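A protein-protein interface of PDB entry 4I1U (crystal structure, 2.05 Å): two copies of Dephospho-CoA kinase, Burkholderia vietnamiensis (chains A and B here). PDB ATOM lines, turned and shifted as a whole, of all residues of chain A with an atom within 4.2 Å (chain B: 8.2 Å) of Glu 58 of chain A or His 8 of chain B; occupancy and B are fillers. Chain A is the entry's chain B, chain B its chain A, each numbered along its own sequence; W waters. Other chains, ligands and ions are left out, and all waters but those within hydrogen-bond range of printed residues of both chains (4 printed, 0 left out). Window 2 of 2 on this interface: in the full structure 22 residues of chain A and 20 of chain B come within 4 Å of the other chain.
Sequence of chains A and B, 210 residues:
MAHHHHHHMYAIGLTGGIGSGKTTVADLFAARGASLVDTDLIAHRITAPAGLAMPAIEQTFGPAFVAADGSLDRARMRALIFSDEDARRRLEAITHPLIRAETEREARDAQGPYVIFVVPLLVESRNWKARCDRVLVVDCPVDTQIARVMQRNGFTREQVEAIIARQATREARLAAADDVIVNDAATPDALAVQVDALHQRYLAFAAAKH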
ATOM      1  N   MET A  54      26.140  19.175  20.169  1.00  0.00           N
ATOM      2  CA  MET A  54      27.095  19.683  19.221  1.00  0.00           C
ATOM      3  C   MET A  54      26.467  20.477  18.077  1.00  0.00           C
ATOM      4  O   MET A  54      27.047  21.479  17.661  1.00  0.00           O
ATOM      5  CB  MET A  54      28.043  18.584  18.721  1.00  0.00           C
ATOM      6  CG  MET A  54      29.032  18.076  19.771  1.00  0.00           C
ATOM      7  SD  MET A  54      29.912  19.389  20.631  1.00  0.00           S
ATOM      8  CE  MET A  54      30.634  20.214  19.235  1.00  0.00           C
ATOM      9  N   PRO A  55      25.306  20.043  17.556  1.00  0.00           N
ATOM     10  CA  PRO A  55      24.718  20.886  16.513  1.00  0.00           C
ATOM     11  C   PRO A  55      24.383  22.301  16.998  1.00  0.00           C
ATOM     12  O   PRO A  55      24.605  23.260  16.290  1.00  0.00           O
ATOM     13  CB  PRO A  55      23.430  20.133  16.149  1.00  0.00           C
ATOM     14  CG  PRO A  55      23.813  18.694  16.341  1.00  0.00           C
ATOM     15  CD  PRO A  55      24.684  18.701  17.580  1.00  0.00           C
ATOM     16  N   ALA A  56      23.876  22.437  18.200  1.00  0.00           N
ATOM     17  CA  ALA A  56      23.506  23.786  18.700  1.00  0.00           C
ATOM     18  C   ALA A  56      24.757  24.615  19.013  1.00  0.00           C
ATOM     19  O   ALA A  56      24.815  25.796  18.753  1.00  0.00           O
ATOM     20  CB  ALA A  56      22.622  23.666  19.939  1.00  0.00           C
ATOM     21  N   ILE A  57      25.789  23.985  19.555  1.00  0.00           N
ATOM     22  CA  ILE A  57      27.058  24.665  19.773  1.00  0.00           C
ATOM     23  C   ILE A  57      27.633  25.178  18.491  1.00  0.00           C
ATOM     24  O   ILE A  57      28.067  26.330  18.418  1.00  0.00           O
ATOM     25  CB  ILE A  57      28.081  23.780  20.520  1.00  0.00           C
ATOM     26  CG1 ILE A  57      27.642  23.647  21.957  1.00  0.00           C
ATOM     27  CG2 ILE A  57      29.474  24.370  20.439  1.00  0.00           C
ATOM     28  CD1 ILE A  57      28.345  22.590  22.740  1.00  0.00           C
ATOM     29  N   GLU A  58      27.626  24.364  17.462  1.00  0.00           N
ATOM     30  CA  GLU A  58      28.174  24.819  16.211  1.00  0.00           C
ATOM     31  C   GLU A  58      27.380  26.018  15.656  1.00  0.00           C
ATOM     32  O   GLU A  58      27.950  26.960  15.065  1.00  0.00           O
ATOM     33  CB  GLU A  58      28.219  23.704  15.167  1.00  0.00           C
ATOM     34  CG  GLU A  58      28.813  24.210  13.865  1.00  0.00           C
ATOM     35  CD  GLU A  58      28.955  23.140  12.812  1.00  0.00           C
ATOM     36  OE1 GLU A  58      29.614  22.107  13.084  1.00  0.00           O
ATOM     37  OE2 GLU A  58      28.393  23.324  11.710  1.00  0.00           O
ATOM     38  N   GLN A  59      26.073  25.948  15.828  1.00  0.00           N
ATOM     39  CA  GLN A  59      25.192  26.989  15.351  1.00  0.00           C
ATOM     40  C   GLN A  59      25.485  28.343  16.011  1.00  0.00           C
ATOM     41  O   GLN A  59      25.559  29.349  15.322  1.00  0.00           O
ATOM     42  CB  GLN A  59      23.739  26.585  15.578  1.00  0.00           C
ATOM     43  CG  GLN A  59      22.740  27.449  14.875  1.00  0.00           C
ATOM     44  CD  GLN A  59      22.671  27.176  13.389  1.00  0.00           C
ATOM     45  OE1 GLN A  59      23.687  27.053  12.723  1.00  0.00           O
ATOM     46  NE2 GLN A  59      21.451  27.020  12.872  1.00  0.00           N
ATOM     47  N   THR A  60      25.647  28.349  17.320  1.00  0.00           N
ATOM     48  CA  THR A  60      25.948  29.579  18.070  1.00  0.00           C
ATOM     49  C   THR A  60      27.413  30.009  18.036  1.00  0.00           C
ATOM     50  O   THR A  60      27.694  31.189  17.878  1.00  0.00           O
ATOM     51  CB  THR A  60      25.487  29.408  19.535  1.00  0.00           C
ATOM     52  OG1 THR A  60      24.068  29.451  19.561  1.00  0.00           O
ATOM     53  CG2 THR A  60      26.041  30.502  20.481  1.00  0.00           C
ATOM     54  N   PHE A  61      28.353  29.074  18.181  1.00  0.00           N
ATOM     55  CA  PHE A  61      29.762  29.440  18.314  1.00  0.00           C
ATOM     56  C   PHE A  61      30.560  29.229  17.037  1.00  0.00           C
ATOM     57  O   PHE A  61      31.657  29.765  16.885  1.00  0.00           O
ATOM     58  CB  PHE A  61      30.371  28.639  19.458  1.00  0.00           C
ATOM     59  CG  PHE A  61      29.796  28.982  20.801  1.00  0.00           C
ATOM     60  CD1 PHE A  61      30.224  30.102  21.485  1.00  0.00           C
ATOM     61  CD2 PHE A  61      28.814  28.192  21.381  1.00  0.00           C
ATOM     62  CE1 PHE A  61      29.703  30.411  22.732  1.00  0.00           C
ATOM     63  CE2 PHE A  61      28.279  28.497  22.612  1.00  0.00           C
ATOM     64  CZ  PHE A  61      28.722  29.615  23.294  1.00  0.00           C
ATOM     65  N   GLY A  62      30.039  28.391  16.145  1.00  0.00           N
ATOM     66  CA  GLY A  62      30.654  28.154  14.853  1.00  0.00           C
ATOM     67  C   GLY A  62      31.717  27.065  14.856  1.00  0.00           C
ATOM     68  O   GLY A  62      32.126  26.578  15.938  1.00  0.00           O
ATOM     69  N   VAL A  66      34.464  23.254  16.977  1.00  0.00           N
ATOM     70  CA  VAL A  66      34.228  21.829  16.665  1.00  0.00           C
ATOM     71  C   VAL A  66      35.532  21.202  16.149  1.00  0.00           C
ATOM     72  O   VAL A  66      36.079  21.598  15.114  1.00  0.00           O
ATOM     73  CB  VAL A  66      33.123  21.680  15.627  1.00  0.00           C
ATOM     74  CG1 VAL A  66      32.898  20.224  15.260  1.00  0.00           C
ATOM     75  CG2 VAL A  66      31.834  22.343  16.109  1.00  0.00           C
ATOM     76  N   HIS B   6      24.064  13.551  10.603  1.00  0.00           N
ATOM     77  CA  HIS B   6      23.861  14.705   9.682  1.00  0.00           C
ATOM     78  C   HIS B   6      24.654  15.901  10.230  1.00  0.00           C
ATOM     79  O   HIS B   6      24.412  16.321  11.354  1.00  0.00           O
ATOM     80  CB  HIS B   6      22.363  15.009   9.606  1.00  0.00           C
ATOM     81  CG  HIS B   6      21.952  15.844   8.429  1.00  0.00           C
ATOM     82  ND1 HIS B   6      21.138  15.362   7.422  1.00  0.00           N
ATOM     83  CD2 HIS B   6      22.197  17.142   8.120  1.00  0.00           C
ATOM     84  CE1 HIS B   6      20.915  16.318   6.538  1.00  0.00           C
ATOM     85  NE2 HIS B   6      21.542  17.410   6.939  1.00  0.00           N
ATOM     86  N   HIS B   7      25.611  16.427   9.464  1.00  0.00           N
ATOM     87  CA  HIS B   7      26.455  17.533   9.956  1.00  0.00           C
ATOM     88  C   HIS B   7      26.054  18.877   9.332  1.00  0.00           C
ATOM     89  O   HIS B   7      25.661  18.958   8.170  1.00  0.00           O
ATOM     90  CB  HIS B   7      27.950  17.283   9.691  1.00  0.00           C
ATOM     91  CG  HIS B   7      28.514  16.053  10.344  1.00  0.00           C
ATOM     92  ND1 HIS B   7      29.716  15.498   9.955  1.00  0.00           N
ATOM     93  CD2 HIS B   7      28.046  15.268  11.345  1.00  0.00           C
ATOM     94  CE1 HIS B   7      29.971  14.434  10.695  1.00  0.00           C
ATOM     95  NE2 HIS B   7      28.972  14.268  11.544  1.00  0.00           N
ATOM     96  N   HIS B   8      26.170  19.942  10.111  1.00  0.00           N
ATOM     97  CA  HIS B   8      25.850  21.289   9.627  1.00  0.00           C
ATOM     98  C   HIS B   8      24.352  21.387   9.232  1.00  0.00           C
ATOM     99  O   HIS B   8      24.026  21.906   8.172  1.00  0.00           O
ATOM    100  CB  HIS B   8      26.712  21.691   8.412  1.00  0.00           C
ATOM    101  CG  HIS B   8      28.140  21.259   8.490  1.00  0.00           C
ATOM    102  ND1 HIS B   8      28.979  21.645   9.518  1.00  0.00           N
ATOM    103  CD2 HIS B   8      28.867  20.447   7.686  1.00  0.00           C
ATOM    104  CE1 HIS B   8      30.173  21.104   9.326  1.00  0.00           C
ATOM    105  NE2 HIS B   8      30.134  20.372   8.225  1.00  0.00           N
ATOM    106  N   MET B   9      23.473  20.871  10.082  1.00  0.00           N
ATOM    107  CA  MET B   9      22.028  20.895   9.865  1.00  0.00           C
ATOM    108  C   MET B   9      21.529  22.321   9.587  1.00  0.00           C
ATOM    109  O   MET B   9      21.885  23.246  10.321  1.00  0.00           O
ATOM    110  CB  MET B   9      21.304  20.268  11.085  1.00  0.00           C
ATOM    111  CG  MET B   9      21.033  21.160  12.300  1.00  0.00           C
ATOM    112  SD  MET B   9      19.746  20.514  13.433  1.00  0.00           S
ATOM    113  CE  MET B   9      20.410  18.906  13.902  1.00  0.00           C
ATOM    114  N   TYR B  10      20.753  22.506   8.532  1.00  0.00           N
ATOM    115  CA  TYR B  10      20.162  23.804   8.215  1.00  0.00           C
ATOM    116  C   TYR B  10      18.770  23.817   8.893  1.00  0.00           C
ATOM    117  O   TYR B  10      18.019  22.838   8.753  1.00  0.00           O
ATOM    118  CB  TYR B  10      20.062  24.007   6.702  1.00  0.00           C
ATOM    119  CG  TYR B  10      19.745  25.442   6.379  1.00  0.00           C
ATOM    120  CD1 TYR B  10      18.433  25.848   6.176  1.00  0.00           C
ATOM    121  CD2 TYR B  10      20.739  26.395   6.315  1.00  0.00           C
ATOM    122  CE1 TYR B  10      18.133  27.173   5.912  1.00  0.00           C
ATOM    123  CE2 TYR B  10      20.462  27.725   6.088  1.00  0.00           C
ATOM    124  CZ  TYR B  10      19.142  28.097   5.869  1.00  0.00           C
ATOM    125  OH  TYR B  10      18.824  29.385   5.582  1.00  0.00           O
ATOM    126  N   ALA B  11      18.479  24.866   9.666  1.00  0.00           N
ATOM    127  CA  ALA B  11      17.284  24.940  10.502  1.00  0.00           C
ATOM    128  C   ALA B  11      16.550  26.241  10.295  1.00  0.00           C
ATOM    129  O   ALA B  11      17.131  27.339  10.404  1.00  0.00           O
ATOM    130  CB  ALA B  11      17.640  24.789  11.963  1.00  0.00           C
ATOM    131  N   PRO B 113      16.250  17.279   3.974  1.00  0.00           N
ATOM    132  CA  PRO B 113      17.390  18.145   3.635  1.00  0.00           C
ATOM    133  C   PRO B 113      17.581  19.354   4.582  1.00  0.00           C
ATOM    134  O   PRO B 113      18.674  19.922   4.652  1.00  0.00           O
ATOM    135  CB  PRO B 113      17.099  18.569   2.206  1.00  0.00           C
ATOM    136  CG  PRO B 113      15.600  18.449   2.079  1.00  0.00           C
ATOM    137  CD  PRO B 113      15.155  17.366   3.002  1.00  0.00           C
ATOM    138  N   TYR B 114      16.546  19.712   5.335  1.00  0.00           N
ATOM    139  CA  TYR B 114      16.664  20.744   6.367  1.00  0.00           C
ATOM    140  C   TYR B 114      15.540  20.508   7.360  1.00  0.00           C
ATOM    141  O   TYR B 114      14.568  19.770   7.073  1.00  0.00           O
ATOM    142  CB  TYR B 114      16.598  22.166   5.768  1.00  0.00           C
ATOM    143  CG  TYR B 114      15.302  22.484   5.019  1.00  0.00           C
ATOM    144  CD1 TYR B 114      15.190  22.254   3.634  1.00  0.00           C
ATOM    145  CD2 TYR B 114      14.230  23.059   5.665  1.00  0.00           C
ATOM    146  CE1 TYR B 114      14.028  22.531   2.964  1.00  0.00           C
ATOM    147  CE2 TYR B 114      13.062  23.377   4.997  1.00  0.00           C
ATOM    148  CZ  TYR B 114      12.968  23.106   3.647  1.00  0.00           C
ATOM    149  OH  TYR B 114      11.820  23.347   2.955  1.00  0.00           O
ATOM    150  N   ALA B 130      19.154  32.456  18.008  1.00  0.00           N
ATOM    151  CA  ALA B 130      20.495  31.971  17.789  1.00  0.00           C
ATOM    152  C   ALA B 130      20.477  30.576  17.158  1.00  0.00           C
ATOM    153  O   ALA B 130      21.327  30.267  16.341  1.00  0.00           O
ATOM    154  CB  ALA B 130      21.251  31.909  19.139  1.00  0.00           C
ATOM    155  N   ARG B 131      19.495  29.740  17.523  1.00  0.00           N
ATOM    156  CA  ARG B 131      19.481  28.355  17.081  1.00  0.00           C
ATOM    157  C   ARG B 131      19.161  28.186  15.588  1.00  0.00           C
ATOM    158  O   ARG B 131      19.599  27.241  14.957  1.00  0.00           O
ATOM    159  CB  ARG B 131      18.460  27.571  17.905  1.00  0.00           C
ATOM    160  CG  ARG B 131      18.362  26.087  17.586  1.00  0.00           C
ATOM    161  CD  ARG B 131      19.725  25.421  17.812  1.00  0.00           C
ATOM    162  NE  ARG B 131      19.738  24.013  17.463  1.00  0.00           N
ATOM    163  CZ  ARG B 131      20.008  23.546  16.251  1.00  0.00           C
ATOM    164  NH1 ARG B 131      20.231  24.391  15.226  1.00  0.00           N
ATOM    165  NH2 ARG B 131      19.995  22.235  16.055  1.00  0.00           N
ATOM    166  N   ASP B 133      18.966  29.115  11.520  1.00  0.00           N
ATOM    167  CA  ASP B 133      19.589  29.820  10.417  1.00  0.00           C
ATOM    168  C   ASP B 133      18.750  30.982   9.904  1.00  0.00           C
ATOM    169  O   ASP B 133      19.307  31.998   9.529  1.00  0.00           O
ATOM    170  CB  ASP B 133      19.890  28.862   9.270  1.00  0.00           C
ATOM    171  CG  ASP B 133      20.953  27.819   9.636  1.00  0.00           C
ATOM    172  OD1 ASP B 133      22.147  28.082   9.419  1.00  0.00           O
ATOM    173  OD2 ASP B 133      20.596  26.725  10.116  1.00  0.00           O
ATOM    174  N   PHE B 205      20.160  27.021   0.461  1.00  0.00           N
ATOM    175  CA  PHE B 205      20.845  27.396   1.684  1.00  0.00           C
ATOM    176  C   PHE B 205      21.433  26.171   2.390  1.00  0.00           C
ATOM    177  O   PHE B 205      22.589  26.193   2.831  1.00  0.00           O
ATOM    178  CB  PHE B 205      19.891  28.156   2.624  1.00  0.00           C
ATOM    179  CG  PHE B 205      19.514  29.566   2.148  1.00  0.00           C
ATOM    180  CD1 PHE B 205      20.457  30.442   1.655  1.00  0.00           C
ATOM    181  CD2 PHE B 205      18.205  30.016   2.284  1.00  0.00           C
ATOM    182  CE1 PHE B 205      20.082  31.738   1.255  1.00  0.00           C
ATOM    183  CE2 PHE B 205      17.832  31.284   1.953  1.00  0.00           C
ATOM    184  CZ  PHE B 205      18.749  32.136   1.397  1.00  0.00           C
ATOM    185  N   ALA B 206      20.650  25.114   2.488  1.00  0.00           N
ATOM    186  CA  ALA B 206      21.093  23.900   3.144  1.00  0.00           C
ATOM    187  C   ALA B 206      22.299  23.298   2.420  1.00  0.00           C
ATOM    188  O   ALA B 206      23.279  22.916   3.057  1.00  0.00           O
ATOM    189  CB  ALA B 206      19.967  22.887   3.194  1.00  0.00           C
ATOM    190  N   ALA B 207      22.218  23.220   1.093  1.00  0.00           N
ATOM    191  CA  ALA B 207      23.306  22.664   0.303  1.00  0.00           C
ATOM    192  C   ALA B 207      24.599  23.471   0.500  1.00  0.00           C
ATOM    193  O   ALA B 207      25.676  22.900   0.599  1.00  0.00           O
ATOM    194  CB  ALA B 207      22.933  22.582  -1.185  1.00  0.00           C
ATOM    195  N   ALA B 208      24.478  24.787   0.596  1.00  0.00           N
ATOM    196  CA  ALA B 208      25.638  25.642   0.821  1.00  0.00           C
ATOM    197  C   ALA B 208      26.242  25.421   2.207  1.00  0.00           C
ATOM    198  O   ALA B 208      27.446  25.428   2.374  1.00  0.00           O
ATOM    199  CB  ALA B 208      25.233  27.089   0.663  1.00  0.00           C
ATOM    200  N   LYS B 209      25.400  25.246   3.206  1.00  0.00           N
ATOM    201  CA  LYS B 209      25.899  25.093   4.573  1.00  0.00           C
ATOM    202  C   LYS B 209      26.723  23.801   4.755  1.00  0.00           C
ATOM    203  O   LYS B 209      27.638  23.746   5.575  1.00  0.00           O
ATOM    204  CB  LYS B 209      24.727  25.101   5.534  1.00  0.00           C
ATOM    205  CG  LYS B 209      25.125  25.025   6.993  1.00  0.00           C
ATOM    206  CD  LYS B 209      24.023  25.463   7.913  1.00  0.00           C
ATOM    207  CE  LYS B 209      24.552  25.518   9.338  1.00  0.00           C
ATOM    208  NZ  LYS B 209      23.455  25.793  10.278  1.00  0.00           N
ATOM    209  N   HIS B 210      26.381  22.768   4.006  1.00  0.00           N
ATOM    210  CA  HIS B 210      27.088  21.499   4.079  1.00  0.00           C
ATOM    211  C   HIS B 210      28.517  21.587   3.574  1.00  0.00           C
ATOM    212  O   HIS B 210      28.888  22.408   2.733  1.00  0.00           O
ATOM    213  CB  HIS B 210      26.337  20.423   3.307  1.00  0.00           C
ATOM    214  CG  HIS B 210      25.160  19.890   4.050  1.00  0.00           C
ATOM    215  ND1 HIS B 210      23.856  20.190   3.709  1.00  0.00           N
ATOM    216  CD2 HIS B 210      25.096  19.090   5.137  1.00  0.00           C
ATOM    217  CE1 HIS B 210      23.040  19.596   4.560  1.00  0.00           C
ATOM    218  NE2 HIS B 210      23.770  18.914   5.428  1.00  0.00           N
ATOM    219  OXT HIS B 210      29.352  20.818   4.049  1.00  0.00           O
HETATM  220  O   HOH W   1      25.874  24.705  12.215  1.00  0.00           O
HETATM  221  O   HOH W   2      23.481  31.848  15.736  1.00  0.00           O
HETATM  222  O   HOH W   3      28.760  19.668  12.107  1.00  0.00           O
HETATM  223  O   HOH W   4      22.075  30.269  13.908  1.00  0.00           O
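The side-chain amino group (NZ) of Lys 209 of chain B is in hydrogen-bond range of the side-chain amide oxygen (OE1) of Gln 59 of chain A.
OE2 of Glu 58 of chain A sits at hydrogen-bond distance from ND1 of His 8 of chain B (2.8 Å).
The side-chain amide nitrogen (NE2) of Gln 59 of chain A is in hydrogen-bond range of the side-chain carboxylate (OD2) of Asp 133 of chain B (2.9 Å).
The backbone carbonyl oxygen (O) of Arg 131 of chain B is in hydrogen-bond range of the side-chain amide nitrogen (NE2) of Gln 59 of chain A.
O of Ala 11 of chain B lies within hydrogen-bond range of N of Asp 133 of chain B, at 2.8 Å.
The side-chain sulfur of Met 9 of chain B is in hydrogen-bond range of the guanidinium group of Arg 131 of chain B.
The side-chain carboxylate (OD1) of Asp 133 of chain B is in salt-bridge range of the side-chain amino group (NZ) of Lys 209 of chain B (2.8 Å).
O of Met 9 of chain B sits at hydrogen-bond distance from NZ of Lys 209 of chain B (3.0 Å).
Among the printed residues, pairs that only touch across the chains: Gln 59 of chain A with Ala 130 of chain B (3.5 Å), Thr 60 of chain A with Ala 130 of chain B (3.8 Å), Ala 56 of chain A with Arg 131 of chain B (3.8 Å) and Pro 55 of chain A with Met 9 of chain B (3.96 Å).
Of the printed residues of chain B, Ala 56 of chain A touches Arg 131.
Of chain B, only His 8 (2.8 Å) comes within 4 Å of Glu 58 of chain A.
Of the printed residues of chain B, Thr 60 of chain A touches Ala 130 (3.8 Å).
His 8 of chain B touches one residue of chain A.
Printed residues of chain A within 4 Å of Ala 130 of chain B: Gln 59 (3.5 Å) and Thr 60 (3.8 Å).
The nearest residue of chain B that does not touch Glu 58 of chain A is Lys 209 of chain B (5.0 Å).
The nearest printed residue of chain B that does not touch Pro 55 of chain A is Arg 131 of chain B (4.03 Å).
Printed residues of chain B that touch a printed residue of chain A: His 8, Met 9, Ala 130, Arg 131, Asp 133 and Lys 209.
Hydrophobic or aromatic side chains of chain B within 4 Å of the printed part of chain A: His 8, Met 9 and Ala 130.
Among the printed residues, 8 pairs touch across the chains.
Among the printed residues, no Asp or Glu carboxylate lies within 4 Å of a Lys or Arg side-chain nitrogen of the other chain.
No position is printed for both chains.
Water W4 lies within hydrogen-bond range of the backbone carbonyl oxygen of Ala 130 of chain B (2.5 Å) and the side-chain amide nitrogen of Gln 59 of chain A (3.5 Å).
Water W2 bridges the backbone carbonyl oxygen (O) of Ala 130 of chain B (2.7 Å) and the backbone carbonyl oxygen (O) of Gln 59 of chain A (3.3 Å).
Water W3 lies within hydrogen-bond range of the side-chain carboxylate of Glu 58 of chain A (2.8 Å) and a ring nitrogen (ND1) of His 8 of chain B (3.3 Å).
Water W1 lies within hydrogen-bond range of the side-chain carboxylate (OE2) of Glu 58 of chain A, the side-chain amide oxygen (OE1) of Gln 59 of chain A and the side-chain amino group (NZ) of Lys 209 of chain B.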
